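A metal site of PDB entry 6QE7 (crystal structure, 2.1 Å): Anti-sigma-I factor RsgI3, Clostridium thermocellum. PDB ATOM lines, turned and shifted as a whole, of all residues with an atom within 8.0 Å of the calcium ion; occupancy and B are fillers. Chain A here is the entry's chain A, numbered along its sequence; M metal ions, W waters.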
ATOM      1  N   GLY A  33       2.110  -5.918   9.424  1.00  0.00           N
ATOM      2  CA  GLY A  33       1.564  -5.208   8.265  1.00  0.00           C
ATOM      3  C   GLY A  33       0.931  -3.899   8.711  1.00  0.00           C
ATOM      4  O   GLY A  33       1.655  -3.132   9.309  1.00  0.00           O
ATOM      5  N   GLU A  34      -0.364  -3.698   8.458  1.00  0.00           N
ATOM      6  CA  GLU A  34      -1.123  -2.517   8.895  1.00  0.00           C
ATOM      7  C   GLU A  34      -2.043  -2.898  10.072  1.00  0.00           C
ATOM      8  O   GLU A  34      -2.989  -2.121  10.405  1.00  0.00           O
ATOM      9  CB  GLU A  34      -1.846  -1.872   7.702  1.00  0.00           C
ATOM     10  CG  GLU A  34      -0.878  -1.307   6.721  1.00  0.00           C
ATOM     11  CD  GLU A  34      -1.508  -0.656   5.515  1.00  0.00           C
ATOM     12  OE1 GLU A  34      -2.240  -1.399   4.782  1.00  0.00           O
ATOM     13  OE2 GLU A  34      -1.273   0.563   5.334  1.00  0.00           O
ATOM     14  N   ASP A  44      -3.530   0.963  15.333  1.00  0.00           N
ATOM     15  CA  ASP A  44      -2.832   2.249  15.527  1.00  0.00           C
ATOM     16  C   ASP A  44      -2.573   2.543  17.022  1.00  0.00           C
ATOM     17  O   ASP A  44      -3.222   1.968  17.916  1.00  0.00           O
ATOM     18  CB  ASP A  44      -3.545   3.412  14.806  1.00  0.00           C
ATOM     19  CG  ASP A  44      -3.570   3.339  13.286  1.00  0.00           C
ATOM     20  OD1 ASP A  44      -2.743   2.613  12.766  1.00  0.00           O
ATOM     21  OD2 ASP A  44      -4.445   4.030  12.619  1.00  0.00           O
ATOM     22  N   THR A  45      -1.596   3.451  17.227  1.00  0.00           N
ATOM     23  CA  THR A  45      -1.148   4.004  18.531  1.00  0.00           C
ATOM     24  C   THR A  45      -1.049   2.874  19.553  1.00  0.00           C
ATOM     25  O   THR A  45      -1.854   2.855  20.484  1.00  0.00           O
ATOM     26  CB  THR A  45      -2.130   5.095  18.986  1.00  0.00           C
ATOM     27  OG1 THR A  45      -3.407   4.472  18.980  1.00  0.00           O
ATOM     28  CG2 THR A  45      -2.186   6.309  18.096  1.00  0.00           C
ATOM     29  N   TYR A  46      -0.061   1.992  19.429  1.00  0.00           N
ATOM     30  CA  TYR A  46       0.184   0.958  20.422  1.00  0.00           C
ATOM     31  C   TYR A  46       1.682   0.938  20.711  1.00  0.00           C
ATOM     32  O   TYR A  46       2.446   1.599  19.945  1.00  0.00           O
ATOM     33  CB  TYR A  46      -0.424  -0.403  20.037  1.00  0.00           C
ATOM     34  CG  TYR A  46      -0.044  -1.000  18.714  1.00  0.00           C
ATOM     35  CD1 TYR A  46       1.075  -1.774  18.588  1.00  0.00           C
ATOM     36  CD2 TYR A  46      -0.887  -0.915  17.593  1.00  0.00           C
ATOM     37  CE1 TYR A  46       1.419  -2.400  17.390  1.00  0.00           C
ATOM     38  CE2 TYR A  46      -0.625  -1.626  16.424  1.00  0.00           C
ATOM     39  CZ  TYR A  46       0.568  -2.323  16.300  1.00  0.00           C
ATOM     40  OH  TYR A  46       0.906  -2.985  15.145  1.00  0.00           O
ATOM     41  N   THR A  68      12.402  -1.194  12.769  1.00  0.00           N
ATOM     42  CA  THR A  68      11.111  -0.833  13.401  1.00  0.00           C
ATOM     43  C   THR A  68      10.377   0.140  12.519  1.00  0.00           C
ATOM     44  O   THR A  68      11.005   1.047  11.916  1.00  0.00           O
ATOM     45  CB  THR A  68      11.248  -0.225  14.789  1.00  0.00           C
ATOM     46  OG1 THR A  68      12.157   0.901  14.913  1.00  0.00           O
ATOM     47  CG2 THR A  68      11.687  -1.260  15.786  1.00  0.00           C
ATOM     48  N   ASP A  69       9.064   0.018  12.607  1.00  0.00           N
ATOM     49  CA  ASP A  69       8.110   1.072  12.263  1.00  0.00           C
ATOM     50  C   ASP A  69       7.038   1.009  13.348  1.00  0.00           C
ATOM     51  O   ASP A  69       6.361  -0.031  13.381  1.00  0.00           O
ATOM     52  CB  ASP A  69       7.596   0.839  10.847  1.00  0.00           C
ATOM     53  CG  ASP A  69       6.459   1.777  10.488  1.00  0.00           C
ATOM     54  OD1 ASP A  69       5.867   2.412  11.444  1.00  0.00           O
ATOM     55  OD2 ASP A  69       6.206   1.901   9.299  1.00  0.00           O
ATOM     56  N   ASP A  70       6.925   2.040  14.271  1.00  0.00           N
ATOM     57  CA  ASP A  70       7.687   3.282  14.203  1.00  0.00           C
ATOM     58  C   ASP A  70       8.938   3.246  15.067  1.00  0.00           C
ATOM     59  O   ASP A  70       9.939   2.673  14.649  1.00  0.00           O
ATOM     60  CB  ASP A  70       6.824   4.477  14.555  1.00  0.00           C
ATOM     61  CG  ASP A  70       5.738   4.655  13.498  1.00  0.00           C
ATOM     62  OD1 ASP A  70       4.738   3.822  13.539  1.00  0.00           O
ATOM     63  OD2 ASP A  70       5.832   5.608  12.716  1.00  0.00           O
ATOM     64  N   GLY A  71       8.898   3.819  16.254  1.00  0.00           N
ATOM     65  CA  GLY A  71      10.141   4.204  16.932  1.00  0.00           C
ATOM     66  C   GLY A  71      10.604   3.149  17.896  1.00  0.00           C
ATOM     67  O   GLY A  71       9.912   2.115  18.139  1.00  0.00           O
ATOM     68  N   LYS A  86      10.438   7.966  17.242  1.00  0.00           N
ATOM     69  CA  LYS A  86       9.891   8.848  16.197  1.00  0.00           C
ATOM     70  C   LYS A  86       9.110   7.994  15.209  1.00  0.00           C
ATOM     71  O   LYS A  86       9.270   6.749  15.208  1.00  0.00           O
ATOM     72  CB  LYS A  86      10.978   9.628  15.446  1.00  0.00           C
ATOM     73  CG  LYS A  86      11.899   8.760  14.605  1.00  0.00           C
ATOM     74  CD  LYS A  86      13.080   9.484  14.057  1.00  0.00           C
ATOM     75  CE  LYS A  86      13.900   8.636  13.107  1.00  0.00           C
ATOM     76  NZ  LYS A  86      14.916   9.502  12.471  1.00  0.00           N
ATOM     77  N   SER A  87       8.343   8.717  14.414  1.00  0.00           N
ATOM     78  CA  SER A  87       7.585   8.284  13.251  1.00  0.00           C
ATOM     79  C   SER A  87       8.623   7.902  12.187  1.00  0.00           C
ATOM     80  O   SER A  87       9.521   8.722  11.828  1.00  0.00           O
ATOM     81  CB  SER A  87       6.649   9.372  12.833  1.00  0.00           C
ATOM     82  OG  SER A  87       5.964   9.017  11.671  1.00  0.00           O
ATOM     83  N   GLN A  88       8.594   6.646  11.756  1.00  0.00           N
ATOM     84  CA  GLN A  88       9.488   6.194  10.686  1.00  0.00           C
ATOM     85  C   GLN A  88       8.900   4.940  10.052  1.00  0.00           C
ATOM     86  O   GLN A  88       8.525   4.051  10.761  1.00  0.00           O
ATOM     87  CB  GLN A  88      10.903   5.872  11.199  1.00  0.00           C
ATOM     88  CG  GLN A  88      10.929   4.960  12.408  1.00  0.00           C
ATOM     89  CD  GLN A  88      12.342   4.607  12.827  1.00  0.00           C
ATOM     90  OE1 GLN A  88      13.241   5.411  12.805  1.00  0.00           O
ATOM     91  NE2 GLN A  88      12.559   3.352  13.210  1.00  0.00           N
ATOM     92  N   SER A  89       8.794   4.948   8.743  1.00  0.00           N
ATOM     93  CA  SER A  89       8.828   3.714   7.949  1.00  0.00           C
ATOM     94  C   SER A  89       9.933   2.800   8.479  1.00  0.00           C
ATOM     95  O   SER A  89      10.889   3.363   9.073  1.00  0.00           O
ATOM     96  CB  SER A  89       9.045   4.061   6.526  1.00  0.00           C
ATOM     97  OG  SER A  89       8.644   2.969   5.759  1.00  0.00           O
ATOM     98  N   ALA A  90       9.871   1.485   8.172  1.00  0.00           N
ATOM     99  CA  ALA A  90      10.816   0.429   8.625  1.00  0.00           C
ATOM    100  C   ALA A  90      12.238   0.880   8.350  1.00  0.00           C
ATOM    101  O   ALA A  90      12.569   1.203   7.202  1.00  0.00           O
ATOM    102  CB  ALA A  90      10.588  -0.878   7.948  1.00  0.00           C
ATOM    103  N   TYR A 111       9.137   0.005  21.947  1.00  0.00           N
ATOM    104  CA  TYR A 111       8.706   0.091  20.543  1.00  0.00           C
ATOM    105  C   TYR A 111       7.376   0.825  20.543  1.00  0.00           C
ATOM    106  O   TYR A 111       6.584   0.563  21.469  1.00  0.00           O
ATOM    107  CB  TYR A 111       8.569  -1.341  19.998  1.00  0.00           C
ATOM    108  CG  TYR A 111       7.685  -1.373  18.796  1.00  0.00           C
ATOM    109  CD1 TYR A 111       8.155  -0.979  17.560  1.00  0.00           C
ATOM    110  CD2 TYR A 111       6.334  -1.627  18.922  1.00  0.00           C
ATOM    111  CE1 TYR A 111       7.340  -0.880  16.463  1.00  0.00           C
ATOM    112  CE2 TYR A 111       5.503  -1.542  17.837  1.00  0.00           C
ATOM    113  CZ  TYR A 111       6.000  -1.160  16.609  1.00  0.00           C
ATOM    114  OH  TYR A 111       5.166  -1.101  15.559  1.00  0.00           O
ATOM    115  N   TYR A 112       7.053   1.573  19.480  1.00  0.00           N
ATOM    116  CA  TYR A 112       5.653   1.978  19.296  1.00  0.00           C
ATOM    117  C   TYR A 112       5.362   2.081  17.802  1.00  0.00           C
ATOM    118  O   TYR A 112       6.258   2.178  16.951  1.00  0.00           O
ATOM    119  CB  TYR A 112       5.375   3.299  20.011  1.00  0.00           C
ATOM    120  CG  TYR A 112       5.815   4.515  19.233  1.00  0.00           C
ATOM    121  CD1 TYR A 112       7.111   4.993  19.285  1.00  0.00           C
ATOM    122  CD2 TYR A 112       4.903   5.241  18.474  1.00  0.00           C
ATOM    123  CE1 TYR A 112       7.500   6.132  18.577  1.00  0.00           C
ATOM    124  CE2 TYR A 112       5.258   6.409  17.805  1.00  0.00           C
ATOM    125  CZ  TYR A 112       6.571   6.881  17.857  1.00  0.00           C
ATOM    126  OH  TYR A 112       6.916   7.955  17.108  1.00  0.00           O
ATOM    127  N   GLN A 113       4.101   1.890  17.525  1.00  0.00           N
ATOM    128  CA  GLN A 113       3.379   2.137  16.268  1.00  0.00           C
ATOM    129  C   GLN A 113       2.519   3.384  16.405  1.00  0.00           C
ATOM    130  O   GLN A 113       1.735   3.550  17.417  1.00  0.00           O
ATOM    131  CB  GLN A 113       2.512   0.901  15.963  1.00  0.00           C
ATOM    132  CG  GLN A 113       1.258   1.234  15.142  1.00  0.00           C
ATOM    133  CD  GLN A 113       1.490   1.516  13.689  1.00  0.00           C
ATOM    134  OE1 GLN A 113       2.488   2.093  13.292  1.00  0.00           O
ATOM    135  NE2 GLN A 113       0.598   0.967  12.849  1.00  0.00           N
ATOM    136  N   HIS A 114       2.627   4.230  15.393  1.00  0.00           N
ATOM    137  CA  HIS A 114       1.722   5.393  15.240  1.00  0.00           C
ATOM    138  C   HIS A 114       0.583   4.980  14.309  1.00  0.00           C
ATOM    139  O   HIS A 114      -0.471   4.595  14.841  1.00  0.00           O
ATOM    140  CB  HIS A 114       2.483   6.671  14.823  1.00  0.00           C
ATOM    141  CG  HIS A 114       1.593   7.871  14.776  1.00  0.00           C
ATOM    142  ND1 HIS A 114       1.669   8.769  13.754  1.00  0.00           N
ATOM    143  CD2 HIS A 114       0.523   8.249  15.553  1.00  0.00           C
ATOM    144  CE1 HIS A 114       0.707   9.693  13.889  1.00  0.00           C
ATOM    145  NE2 HIS A 114      -0.006   9.390  15.008  1.00  0.00           N
ATOM    146  N   VAL A 115       0.801   4.997  12.996  1.00  0.00           N
ATOM    147  CA  VAL A 115      -0.229   4.688  11.980  1.00  0.00           C
ATOM    148  C   VAL A 115       0.346   3.857  10.829  1.00  0.00           C
ATOM    149  O   VAL A 115       1.537   3.505  10.816  1.00  0.00           O
ATOM    150  CB  VAL A 115      -0.864   5.993  11.462  1.00  0.00           C
ATOM    151  CG1 VAL A 115      -1.637   6.769  12.563  1.00  0.00           C
ATOM    152  CG2 VAL A 115       0.122   6.877  10.751  1.00  0.00           C
ATOM    153  N   ARG A 116      -0.514   3.479   9.884  1.00  0.00           N
ATOM    154  CA  ARG A 116      -0.030   2.722   8.714  1.00  0.00           C
ATOM    155  C   ARG A 116       0.664   1.450   9.192  1.00  0.00           C
ATOM    156  O   ARG A 116       0.025   0.633   9.936  1.00  0.00           O
ATOM    157  CB  ARG A 116       0.819   3.643   7.878  1.00  0.00           C
ATOM    158  CG  ARG A 116      -0.003   4.889   7.579  1.00  0.00           C
ATOM    159  CD  ARG A 116       0.519   5.615   6.369  1.00  0.00           C
ATOM    160  NE  ARG A 116      -0.247   6.854   6.206  1.00  0.00           N
ATOM    161  CZ  ARG A 116      -0.621   7.359   5.033  1.00  0.00           C
ATOM    162  NH1 ARG A 116      -0.320   6.736   3.915  1.00  0.00           N
ATOM    163  NH2 ARG A 116      -1.244   8.520   4.996  1.00  0.00           N
ATOM    164  N   ALA A 117       1.823   1.193   8.653  1.00  0.00           N
ATOM    165  CA  ALA A 117       2.484  -0.125   8.802  1.00  0.00           C
ATOM    166  C   ALA A 117       3.098  -0.227  10.200  1.00  0.00           C
ATOM    167  O   ALA A 117       3.405   0.810  10.795  1.00  0.00           O
ATOM    168  CB  ALA A 117       3.500  -0.274   7.709  1.00  0.00           C
ATOM    169  N   ALA A 118       3.299  -1.428  10.717  1.00  0.00           N
ATOM    170  CA  ALA A 118       3.878  -1.681  12.063  1.00  0.00           C
ATOM    171  C   ALA A 118       4.757  -2.938  12.006  1.00  0.00           C
ATOM    172  O   ALA A 118       4.252  -3.998  11.506  1.00  0.00           O
ATOM    173  CB  ALA A 118       2.757  -1.769  13.105  1.00  0.00           C
ATOM    174  N   SER A 119       6.009  -2.842  12.464  1.00  0.00           N
ATOM    175  CA  SER A 119       6.943  -3.993  12.576  1.00  0.00           C
ATOM    176  C   SER A 119       8.023  -3.738  13.617  1.00  0.00           C
ATOM    177  O   SER A 119       8.364  -2.577  13.872  1.00  0.00           O
ATOM    178  CB  SER A 119       7.593  -4.315  11.222  1.00  0.00           C
ATOM    179  OG  SER A 119       8.169  -3.174  10.591  1.00  0.00           O
HETATM  180 CA    CA M   1       3.654   2.966  11.559  1.00  0.00          CA
HETATM  181  O   HOH W   1       4.523   3.969   9.159  1.00  0.00           O
HETATM  182  O   HOH W   2       3.869   5.588  10.778  1.00  0.00           O
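The side-chain amide nitrogen of Gln 113 lies within hydrogen-bond range of the backbone carbonyl oxygen of Arg 116, at 3.0 Å. The backbone carbonyl oxygen (O) of Asp 70 is in hydrogen-bond range of the side-chain amide nitrogen (NE2) of Gln 88 (3.1 Å). The backbone carbonyl oxygen (O) of Asp 70 sits at hydrogen-bond distance from the side-chain hydroxyl (OG1) of Thr 68. N of Asp 69 is in hydrogen-bond range of O of Ser 119 (3.0 Å). The backbone carbonyl oxygen (O) of Asp 69 is in hydrogen-bond range of the side-chain hydroxyl (OH) of Tyr 111 (2.7 Å). The backbone NH (N) of Gln 113 is in hydrogen-bond range of the backbone carbonyl oxygen (O) of Tyr 46, at 2.9 Å. OD1 of Asp 70 lies close to N of His 114 (2.8 Å). O of Gln 113 sits close to N of Thr 45 (3.3 Å).
Of the 23 residues printed, 5 come within 4 Å of the calcium ion. Along chain A the residues within 4 Å of the calcium ion span positions 69 to 117. The nearest printed residue that does not touch the calcium ion is Arg 116 (4.1 Å).
The calcium ion is bound by the side-chain amide oxygen of Gln 113 (2.3 Å), the side-chain carboxylate of Asp 69 (2.3 Å), the backbone carbonyl oxygen of Ala 117 (2.3 Å), the backbone carbonyl oxygen of Val 115 (2.3 Å), the side-chain carboxylate of Asp 70 (2.4 Å), water W1 (2.7 Å) and water W2 (2.7 Å). The calcium ion has seven donor atoms within binding distance.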
